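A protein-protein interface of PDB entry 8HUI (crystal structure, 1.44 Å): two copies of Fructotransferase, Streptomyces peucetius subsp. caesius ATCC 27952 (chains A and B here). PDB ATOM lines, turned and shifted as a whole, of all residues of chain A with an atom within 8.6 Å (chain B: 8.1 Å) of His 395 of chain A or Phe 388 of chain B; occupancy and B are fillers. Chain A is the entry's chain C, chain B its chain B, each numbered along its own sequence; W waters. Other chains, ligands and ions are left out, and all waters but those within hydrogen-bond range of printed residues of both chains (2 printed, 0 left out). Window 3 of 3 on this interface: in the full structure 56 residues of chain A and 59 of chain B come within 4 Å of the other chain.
Position printed for both chains: 391.
Of the 7 pairs that touch across the chains among the printed residues, none has its exchanged pair printed and touching as well.
Water W1 lies within hydrogen-bond range of NE2 of His 395 of chain A (2.9 Å), O of His 387 of chain B (3.2 Å) and O of Thr 385 of chain B (3.3 Å).
Water W2 lies within hydrogen-bond range of OD1 of Asn 386 of chain B (3.0 Å), N of His 387 of chain B (3.2 Å) and NE2 of His 395 of chain A (3.4 Å).
CG2 of Thr 392 of chain A touches CD of Arg 370 of chain B, 3.5 Å away.
Pro 393 of chain A touches Leu 372 of chain B.
Pro 393 of chain A touches Phe 388 of chain B.
CG2 of Val 390 of chain B touches CG of Pro 393 of chain A (3.8 Å).
Phe 388 of chain B touches Ser 394 of chain A.
CE2 of Phe 388 of chain B touches NE2 of His 395 of chain A, at 3.3 Å.
His 395 of chain A touches just one residue of chain B: Phe 388 (3.3 Å).
Printed residues of chain A within 4 Å of Phe 388 of chain B: Pro 393 (3.5 Å), Ser 394 (3.7 Å) and His 395 (3.3 Å).
Of chain B, only Phe 388 comes within 4 Å of Ser 394 of chain A.
Printed residues of chain A within 4 Å of Val 390 of chain B: Pro 393 (3.8 Å).
Printed residues of chain A within 4 Å of Leu 372 of chain B: Pro 393 (3.7 Å).
Printed residues of chain A within 4 Å of Arg 370 of chain B: Thr 392 and Pro 393.
Printed residues of chain B within 4 Å of Pro 393 of chain A: Arg 370, Leu 372, Phe 388 and Val 390.
The nearest residue of chain B that does not touch His 395 of chain A is His 387 of chain B (5.0 Å).
The nearest residue of chain A that does not touch Phe 388 of chain B is Thr 392 of chain A (6.5 Å).
The nearest printed residue of chain A that does not touch Arg 370 of chain B is Thr 376 of chain A (4.2 Å).
The guanidinium group (NE) of Arg 370 of chain B lies within hydrogen-bond range of the backbone carbonyl oxygen (O) of Pro 393 of chain A.
Printed residues of chain A that touch a printed residue of chain B: Thr 392, Pro 393, Ser 394 and His 395.
Of the 21 printed residues of chain B, 4 touch a printed residue of chain A.
OD1 of Asn 344 of chain B is in hydrogen-bond range of NH1 of Arg 370 of chain B.
The backbone carbonyl oxygen (O) of Asn 345 of chain B is in hydrogen-bond range of the backbone NH (N) of Arg 370 of chain B (2.9 Å).
The backbone carbonyl oxygen (O) of Thr 369 of chain B sits at hydrogen-bond distance from the backbone NH (N) of Phe 388 of chain B (2.8 Å).
The backbone NH of Val 371 of chain B sits at hydrogen-bond distance from the backbone carbonyl oxygen of Phe 388 of chain B.
N of Val 390 of chain B lies within hydrogen-bond range of O of Val 371 of chain B.
N of His 373 of chain B lies within hydrogen-bond range of O of Val 390 of chain B (2.9 Å).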
ATOM      1  N   THR A 376      22.332  -2.088   2.749  1.00  0.00           N
ATOM      2  CA  THR A 376      21.954  -0.963   3.585  1.00  0.00           C
ATOM      3  C   THR A 376      23.156  -0.024   3.694  1.00  0.00           C
ATOM      4  O   THR A 376      24.274  -0.367   3.292  1.00  0.00           O
ATOM      5  CB  THR A 376      21.635  -1.448   4.991  1.00  0.00           C
ATOM      6  OG1 THR A 376      22.830  -2.033   5.522  1.00  0.00           O
ATOM      7  CG2 THR A 376      20.479  -2.452   5.022  1.00  0.00           C
ATOM      8  N   THR A 377      22.938   1.162   4.264  1.00  0.00           N
ATOM      9  CA  THR A 377      24.055   2.070   4.507  1.00  0.00           C
ATOM     10  C   THR A 377      25.172   1.373   5.277  1.00  0.00           C
ATOM     11  O   THR A 377      26.359   1.529   4.950  1.00  0.00           O
ATOM     12  CB  THR A 377      23.548   3.298   5.263  1.00  0.00           C
ATOM     13  OG1 THR A 377      22.613   4.001   4.437  1.00  0.00           O
ATOM     14  CG2 THR A 377      24.706   4.226   5.627  1.00  0.00           C
ATOM     15  N   ALA A 378      24.811   0.621   6.318  1.00  0.00           N
ATOM     16  CA  ALA A 378      25.802  -0.063   7.137  1.00  0.00           C
ATOM     17  C   ALA A 378      26.548  -1.144   6.374  1.00  0.00           C
ATOM     18  O   ALA A 378      27.623  -1.560   6.810  1.00  0.00           O
ATOM     19  CB  ALA A 378      25.127  -0.689   8.353  1.00  0.00           C
ATOM     20  N   ALA A 391      19.959   3.003  -1.140  1.00  0.00           N
ATOM     21  CA  ALA A 391      20.179   2.072  -0.048  1.00  0.00           C
ATOM     22  C   ALA A 391      19.012   1.124   0.127  1.00  0.00           C
ATOM     23  O   ALA A 391      17.845   1.504   0.002  1.00  0.00           O
ATOM     24  CB  ALA A 391      20.374   2.836   1.263  1.00  0.00           C
ATOM     25  N   THR A 392      19.328  -0.113   0.472  1.00  0.00           N
ATOM     26  CA  THR A 392      18.314  -0.955   1.061  1.00  0.00           C
ATOM     27  C   THR A 392      17.879  -0.287   2.362  1.00  0.00           C
ATOM     28  O   THR A 392      18.741   0.113   3.160  1.00  0.00           O
ATOM     29  CB  THR A 392      18.929  -2.310   1.358  1.00  0.00           C
ATOM     30  OG1 THR A 392      19.420  -2.872   0.136  1.00  0.00           O
ATOM     31  CG2 THR A 392      17.943  -3.255   1.985  1.00  0.00           C
ATOM     32  N   PRO A 393      16.580  -0.118   2.604  1.00  0.00           N
ATOM     33  CA  PRO A 393      16.163   0.644   3.791  1.00  0.00           C
ATOM     34  C   PRO A 393      16.676   0.057   5.104  1.00  0.00           C
ATOM     35  O   PRO A 393      16.793  -1.157   5.285  1.00  0.00           O
ATOM     36  CB  PRO A 393      14.634   0.612   3.715  1.00  0.00           C
ATOM     37  CG  PRO A 393      14.346   0.473   2.237  1.00  0.00           C
ATOM     38  CD  PRO A 393      15.445  -0.388   1.690  1.00  0.00           C
ATOM     39  N   SER A 394      16.965   0.959   6.039  1.00  0.00           N
ATOM     40  CA  SER A 394      17.401   0.597   7.377  1.00  0.00           C
ATOM     41  C   SER A 394      17.033   1.750   8.303  1.00  0.00           C
ATOM     42  O   SER A 394      16.686   2.841   7.853  1.00  0.00           O
ATOM     43  CB  SER A 394      18.895   0.281   7.432  1.00  0.00           C
ATOM     44  OG  SER A 394      19.667   1.443   7.216  1.00  0.00           O
ATOM     45  N   HIS A 395      17.118   1.505   9.605  1.00  0.00           N
ATOM     46  CA  HIS A 395      16.667   2.478  10.595  1.00  0.00           C
ATOM     47  C   HIS A 395      17.822   3.294  11.160  1.00  0.00           C
ATOM     48  O   HIS A 395      18.998   2.998  10.956  1.00  0.00           O
ATOM     49  CB  HIS A 395      15.897   1.752  11.703  1.00  0.00           C
ATOM     50  CG  HIS A 395      14.529   1.324  11.283  1.00  0.00           C
ATOM     51  ND1 HIS A 395      13.668   2.169  10.616  1.00  0.00           N
ATOM     52  CD2 HIS A 395      13.884   0.142  11.402  1.00  0.00           C
ATOM     53  CE1 HIS A 395      12.545   1.524  10.349  1.00  0.00           C
ATOM     54  NE2 HIS A 395      12.644   0.298  10.832  1.00  0.00           N
ATOM     55  N   HIS A 396      17.458   4.363  11.876  1.00  0.00           N
ATOM     56  CA  HIS A 396      18.394   5.130  12.704  1.00  0.00           C
ATOM     57  C   HIS A 396      19.419   5.891  11.857  1.00  0.00           C
ATOM     58  O   HIS A 396      20.613   5.874  12.147  1.00  0.00           O
ATOM     59  CB  HIS A 396      19.090   4.252  13.752  1.00  0.00           C
ATOM     60  CG  HIS A 396      18.161   3.355  14.517  1.00  0.00           C
ATOM     61  ND1 HIS A 396      17.045   3.811  15.186  1.00  0.00           N
ATOM     62  CD2 HIS A 396      18.183   2.013  14.694  1.00  0.00           C
ATOM     63  CE1 HIS A 396      16.426   2.785  15.752  1.00  0.00           C
ATOM     64  NE2 HIS A 396      17.092   1.686  15.462  1.00  0.00           N
ATOM     65  N   HIS A 397      18.930   6.587  10.826  1.00  0.00           N
ATOM     66  CA  HIS A 397      19.801   7.477  10.060  1.00  0.00           C
ATOM     67  C   HIS A 397      20.392   8.555  10.965  1.00  0.00           C
ATOM     68  O   HIS A 397      21.569   8.921  10.838  1.00  0.00           O
ATOM     69  CB  HIS A 397      19.028   8.163   8.928  1.00  0.00           C
ATOM     70  CG  HIS A 397      18.281   7.230   8.020  1.00  0.00           C
ATOM     71  ND1 HIS A 397      17.608   7.675   6.901  1.00  0.00           N
ATOM     72  CD2 HIS A 397      18.116   5.884   8.048  1.00  0.00           C
ATOM     73  CE1 HIS A 397      17.049   6.647   6.286  1.00  0.00           C
ATOM     74  NE2 HIS A 397      17.342   5.549   6.961  1.00  0.00           N
ATOM     75  N   HIS A 398      19.586   9.077  11.881  1.00  0.00           N
ATOM     76  CA  HIS A 398      19.981  10.179  12.742  1.00  0.00           C
ATOM     77  C   HIS A 398      20.251   9.681  14.151  1.00  0.00           C
ATOM     78  O   HIS A 398      19.789   8.611  14.559  1.00  0.00           O
ATOM     79  CB  HIS A 398      18.915  11.272  12.737  1.00  0.00           C
ATOM     80  CG  HIS A 398      18.633  11.805  11.372  1.00  0.00           C
ATOM     81  ND1 HIS A 398      19.621  12.342  10.574  1.00  0.00           N
ATOM     82  CD2 HIS A 398      17.490  11.852  10.646  1.00  0.00           C
ATOM     83  CE1 HIS A 398      19.093  12.717   9.421  1.00  0.00           C
ATOM     84  NE2 HIS A 398      17.801  12.445   9.447  1.00  0.00           N
ATOM     85  N   ASN B 344      13.295 -10.226   8.957  1.00  0.00           N
ATOM     86  CA  ASN B 344      14.255  -9.804   7.941  1.00  0.00           C
ATOM     87  C   ASN B 344      14.043 -10.513   6.612  1.00  0.00           C
ATOM     88  O   ASN B 344      14.987 -10.668   5.829  1.00  0.00           O
ATOM     89  CB  ASN B 344      15.710  -9.931   8.418  1.00  0.00           C
ATOM     90  CG  ASN B 344      16.250  -8.618   8.986  1.00  0.00           C
ATOM     91  OD1 ASN B 344      16.556  -7.688   8.238  1.00  0.00           O
ATOM     92  ND2 ASN B 344      16.339  -8.530  10.306  1.00  0.00           N
ATOM     93  N   ASN B 345      12.813 -10.921   6.336  1.00  0.00           N
ATOM     94  CA  ASN B 345      12.526 -11.407   4.984  1.00  0.00           C
ATOM     95  C   ASN B 345      12.586 -10.250   3.994  1.00  0.00           C
ATOM     96  O   ASN B 345      12.359  -9.091   4.353  1.00  0.00           O
ATOM     97  CB  ASN B 345      11.171 -12.117   4.948  1.00  0.00           C
ATOM     98  CG  ASN B 345      11.206 -13.411   5.704  1.00  0.00           C
ATOM     99  OD1 ASN B 345      11.847 -14.377   5.275  1.00  0.00           O
ATOM    100  ND2 ASN B 345      10.539 -13.451   6.857  1.00  0.00           N
ATOM    101  N   LEU B 347      11.648  -9.022  -0.077  1.00  0.00           N
ATOM    102  CA  LEU B 347      10.930  -9.147  -1.343  1.00  0.00           C
ATOM    103  C   LEU B 347      11.338  -7.959  -2.193  1.00  0.00           C
ATOM    104  O   LEU B 347      11.186  -6.813  -1.759  1.00  0.00           O
ATOM    105  CB  LEU B 347       9.422  -9.067  -1.127  1.00  0.00           C
ATOM    106  CG  LEU B 347       8.666 -10.332  -0.738  1.00  0.00           C
ATOM    107  CD1 LEU B 347       9.158 -10.935   0.566  1.00  0.00           C
ATOM    108  CD2 LEU B 347       7.192 -10.026  -0.616  1.00  0.00           C
ATOM    109  N   LEU B 362       1.672  -9.001   5.613  1.00  0.00           N
ATOM    110  CA  LEU B 362       2.702  -9.121   6.644  1.00  0.00           C
ATOM    111  C   LEU B 362       1.992  -9.332   7.974  1.00  0.00           C
ATOM    112  O   LEU B 362       1.346  -8.413   8.491  1.00  0.00           O
ATOM    113  CB  LEU B 362       3.569  -7.873   6.708  1.00  0.00           C
ATOM    114  CG  LEU B 362       4.199  -7.433   5.383  1.00  0.00           C
ATOM    115  CD1 LEU B 362       5.109  -6.266   5.617  1.00  0.00           C
ATOM    116  CD2 LEU B 362       4.983  -8.587   4.723  1.00  0.00           C
ATOM    117  N   THR B 367       8.850  -9.094  11.646  1.00  0.00           N
ATOM    118  CA  THR B 367       9.738  -7.977  11.913  1.00  0.00           C
ATOM    119  C   THR B 367      10.661  -7.773  10.719  1.00  0.00           C
ATOM    120  O   THR B 367      11.144  -8.740  10.121  1.00  0.00           O
ATOM    121  CB  THR B 367      10.576  -8.213  13.178  1.00  0.00           C
ATOM    122  OG1 THR B 367      11.242  -9.469  13.088  1.00  0.00           O
ATOM    123  CG2 THR B 367       9.683  -8.226  14.410  1.00  0.00           C
ATOM    124  N   ALA B 368      10.907  -6.501  10.390  1.00  0.00           N
ATOM    125  CA  ALA B 368      11.965  -6.106   9.470  1.00  0.00           C
ATOM    126  C   ALA B 368      11.773  -6.666   8.067  1.00  0.00           C
ATOM    127  O   ALA B 368      12.758  -6.864   7.343  1.00  0.00           O
ATOM    128  CB  ALA B 368      13.346  -6.492  10.011  1.00  0.00           C
ATOM    129  N   THR B 369      10.525  -6.907   7.651  1.00  0.00           N
ATOM    130  CA  THR B 369      10.316  -7.316   6.266  1.00  0.00           C
ATOM    131  C   THR B 369      10.565  -6.130   5.346  1.00  0.00           C
ATOM    132  O   THR B 369      10.110  -5.014   5.610  1.00  0.00           O
ATOM    133  CB  THR B 369       8.886  -7.811   6.030  1.00  0.00           C
ATOM    134  OG1 THR B 369       8.555  -8.790   7.015  1.00  0.00           O
ATOM    135  CG2 THR B 369       8.777  -8.461   4.645  1.00  0.00           C
ATOM    136  N   ARG B 370      11.284  -6.363   4.259  1.00  0.00           N
ATOM    137  CA  ARG B 370      11.513  -5.354   3.235  1.00  0.00           C
ATOM    138  C   ARG B 370      10.719  -5.729   2.003  1.00  0.00           C
ATOM    139  O   ARG B 370      10.782  -6.872   1.551  1.00  0.00           O
ATOM    140  CB  ARG B 370      12.996  -5.275   2.890  1.00  0.00           C
ATOM    141  CG  ARG B 370      13.778  -4.483   3.926  1.00  0.00           C
ATOM    142  CD  ARG B 370      15.245  -4.669   3.808  1.00  0.00           C
ATOM    143  NE  ARG B 370      15.886  -3.901   4.866  1.00  0.00           N
ATOM    144  CZ  ARG B 370      16.258  -4.412   6.032  1.00  0.00           C
ATOM    145  NH1 ARG B 370      15.997  -5.659   6.349  1.00  0.00           N
ATOM    146  NH2 ARG B 370      16.867  -3.626   6.912  1.00  0.00           N
ATOM    147  N   VAL B 371       9.974  -4.770   1.468  1.00  0.00           N
ATOM    148  CA  VAL B 371       9.121  -4.963   0.301  1.00  0.00           C
ATOM    149  C   VAL B 371       9.482  -3.830  -0.643  1.00  0.00           C
ATOM    150  O   VAL B 371       9.063  -2.691  -0.426  1.00  0.00           O
ATOM    151  CB  VAL B 371       7.630  -4.958   0.650  1.00  0.00           C
ATOM    152  CG1 VAL B 371       6.792  -5.375  -0.574  1.00  0.00           C
ATOM    153  CG2 VAL B 371       7.350  -5.923   1.812  1.00  0.00           C
ATOM    154  N   LEU B 372      10.295  -4.128  -1.667  1.00  0.00           N
ATOM    155  CA  LEU B 372      11.003  -3.126  -2.459  1.00  0.00           C
ATOM    156  C   LEU B 372      10.662  -3.343  -3.929  1.00  0.00           C
ATOM    157  O   LEU B 372      11.126  -4.313  -4.537  1.00  0.00           O
ATOM    158  CB  LEU B 372      12.511  -3.250  -2.264  1.00  0.00           C
ATOM    159  CG  LEU B 372      13.001  -3.370  -0.826  1.00  0.00           C
ATOM    160  CD1 LEU B 372      14.508  -3.565  -0.784  1.00  0.00           C
ATOM    161  CD2 LEU B 372      12.603  -2.169   0.032  1.00  0.00           C
ATOM    162  N   HIS B 373       9.862  -2.457  -4.508  1.00  0.00           N
ATOM    163  CA  HIS B 373       9.391  -2.634  -5.883  1.00  0.00           C
ATOM    164  C   HIS B 373       8.826  -4.032  -6.086  1.00  0.00           C
ATOM    165  O   HIS B 373       9.086  -4.693  -7.098  1.00  0.00           O
ATOM    166  CB  HIS B 373      10.501  -2.359  -6.902  1.00  0.00           C
ATOM    167  CG  HIS B 373      10.988  -0.947  -6.905  1.00  0.00           C
ATOM    168  ND1 HIS B 373      12.193  -0.588  -7.468  1.00  0.00           N
ATOM    169  CD2 HIS B 373      10.436   0.194  -6.426  1.00  0.00           C
ATOM    170  CE1 HIS B 373      12.366   0.719  -7.321  1.00  0.00           C
ATOM    171  NE2 HIS B 373      11.309   1.219  -6.706  1.00  0.00           N
ATOM    172  N   LEU B 380      -0.108  -4.140  -0.752  1.00  0.00           N
ATOM    173  CA  LEU B 380       0.504  -4.449   0.531  1.00  0.00           C
ATOM    174  C   LEU B 380      -0.553  -4.318   1.614  1.00  0.00           C
ATOM    175  O   LEU B 380      -1.219  -3.283   1.711  1.00  0.00           O
ATOM    176  CB  LEU B 380       1.656  -3.507   0.838  1.00  0.00           C
ATOM    177  CG  LEU B 380       2.372  -3.795   2.158  1.00  0.00           C
ATOM    178  CD1 LEU B 380       3.094  -5.120   2.135  1.00  0.00           C
ATOM    179  CD2 LEU B 380       3.348  -2.696   2.458  1.00  0.00           C
ATOM    180  N   ALA B 382       0.063  -4.627   5.334  1.00  0.00           N
ATOM    181  CA  ALA B 382       1.004  -4.771   6.433  1.00  0.00           C
ATOM    182  C   ALA B 382       0.245  -4.699   7.749  1.00  0.00           C
ATOM    183  O   ALA B 382      -0.341  -3.661   8.076  1.00  0.00           O
ATOM    184  CB  ALA B 382       2.026  -3.645   6.376  1.00  0.00           C
ATOM    185  N   THR B 384       1.670  -5.143  10.629  1.00  0.00           N
ATOM    186  CA  THR B 384       2.611  -4.588  11.592  1.00  0.00           C
ATOM    187  C   THR B 384       3.267  -3.363  10.969  1.00  0.00           C
ATOM    188  O   THR B 384       3.544  -3.339   9.762  1.00  0.00           O
ATOM    189  CB  THR B 384       3.695  -5.600  12.005  1.00  0.00           C
ATOM    190  OG1 THR B 384       4.672  -4.936  12.815  1.00  0.00           O
ATOM    191  CG2 THR B 384       4.382  -6.233  10.818  1.00  0.00           C
ATOM    192  N   THR B 385       3.538  -2.361  11.800  1.00  0.00           N
ATOM    193  CA  THR B 385       4.316  -1.200  11.402  1.00  0.00           C
ATOM    194  C   THR B 385       5.805  -1.507  11.323  1.00  0.00           C
ATOM    195  O   THR B 385       6.583  -0.664  10.867  1.00  0.00           O
ATOM    196  CB  THR B 385       4.025  -0.056  12.375  1.00  0.00           C
ATOM    197  OG1 THR B 385       4.064  -0.558  13.717  1.00  0.00           O
ATOM    198  CG2 THR B 385       2.651   0.528  12.143  1.00  0.00           C
ATOM    199  N   ASN B 386       6.219  -2.713  11.710  1.00  0.00           N
ATOM    200  CA  ASN B 386       7.624  -3.109  11.654  1.00  0.00           C
ATOM    201  C   ASN B 386       7.937  -3.738  10.294  1.00  0.00           C
ATOM    202  O   ASN B 386       8.069  -4.956  10.149  1.00  0.00           O
ATOM    203  CB  ASN B 386       7.933  -4.080  12.779  1.00  0.00           C
ATOM    204  CG  ASN B 386       9.406  -4.311  12.963  1.00  0.00           C
ATOM    205  OD1 ASN B 386      10.217  -4.010  12.079  1.00  0.00           O
ATOM    206  ND2 ASN B 386       9.773  -4.842  14.124  1.00  0.00           N
ATOM    207  N   HIS B 387       8.058  -2.880   9.288  1.00  0.00           N
ATOM    208  CA  HIS B 387       8.467  -3.285   7.951  1.00  0.00           C
ATOM    209  C   HIS B 387       9.013  -2.061   7.233  1.00  0.00           C
ATOM    210  O   HIS B 387       8.890  -0.928   7.706  1.00  0.00           O
ATOM    211  CB  HIS B 387       7.287  -3.879   7.167  1.00  0.00           C
ATOM    212  CG  HIS B 387       6.264  -2.860   6.757  1.00  0.00           C
ATOM    213  ND1 HIS B 387       5.277  -2.413   7.607  1.00  0.00           N
ATOM    214  CD2 HIS B 387       6.097  -2.172   5.601  1.00  0.00           C
ATOM    215  CE1 HIS B 387       4.531  -1.516   6.986  1.00  0.00           C
ATOM    216  NE2 HIS B 387       5.014  -1.345   5.769  1.00  0.00           N
ATOM    217  N   PHE B 388       9.628  -2.303   6.082  1.00  0.00           N
ATOM    218  CA  PHE B 388      10.073  -1.249   5.176  1.00  0.00           C
ATOM    219  C   PHE B 388       9.351  -1.433   3.850  1.00  0.00           C
ATOM    220  O   PHE B 388       9.416  -2.514   3.262  1.00  0.00           O
ATOM    221  CB  PHE B 388      11.571  -1.335   4.897  1.00  0.00           C
ATOM    222  CG  PHE B 388      12.456  -1.353   6.120  1.00  0.00           C
ATOM    223  CD1 PHE B 388      12.847  -2.543   6.706  1.00  0.00           C
ATOM    224  CD2 PHE B 388      12.944  -0.166   6.634  1.00  0.00           C
ATOM    225  CE1 PHE B 388      13.700  -2.545   7.815  1.00  0.00           C
ATOM    226  CE2 PHE B 388      13.791  -0.164   7.725  1.00  0.00           C
ATOM    227  CZ  PHE B 388      14.162  -1.342   8.314  1.00  0.00           C
ATOM    228  N   MET B 389       8.720  -0.381   3.352  1.00  0.00           N
ATOM    229  CA  MET B 389       8.041  -0.384   2.060  1.00  0.00           C
ATOM    230  C   MET B 389       8.710   0.644   1.150  1.00  0.00           C
ATOM    231  O   MET B 389       8.821   1.826   1.510  1.00  0.00           O
ATOM    232  CB  MET B 389       6.561  -0.060   2.215  1.00  0.00           C
ATOM    233  CG  MET B 389       5.864   0.243   0.888  1.00  0.00           C
ATOM    234  SD  MET B 389       5.739  -1.258  -0.126  1.00  0.00           S
ATOM    235  CE  MET B 389       4.110  -1.042  -0.827  1.00  0.00           C
ATOM    236  N   VAL B 390       9.148   0.194  -0.023  1.00  0.00           N
ATOM    237  CA  VAL B 390       9.488   1.069  -1.145  1.00  0.00           C
ATOM    238  C   VAL B 390       8.534   0.649  -2.258  1.00  0.00           C
ATOM    239  O   VAL B 390       8.721  -0.394  -2.893  1.00  0.00           O
ATOM    240  CB  VAL B 390      10.959   0.974  -1.569  1.00  0.00           C
ATOM    241  CG1 VAL B 390      11.197   1.804  -2.825  1.00  0.00           C
ATOM    242  CG2 VAL B 390      11.831   1.481  -0.445  1.00  0.00           C
ATOM    243  N   ALA B 391       7.445   1.391  -2.425  1.00  0.00           N
ATOM    244  CA  ALA B 391       6.320   0.934  -3.230  1.00  0.00           C
ATOM    245  C   ALA B 391       6.679   0.823  -4.705  1.00  0.00           C
ATOM    246  O   ALA B 391       7.376   1.674  -5.248  1.00  0.00           O
ATOM    247  CB  ALA B 391       5.169   1.923  -3.105  1.00  0.00           C
HETATM  248  O   HOH W   1       9.869  -0.404  10.758  1.00  0.00           O
HETATM  249  O   HOH W   2      11.261  -2.524   9.656  1.00  0.00           O
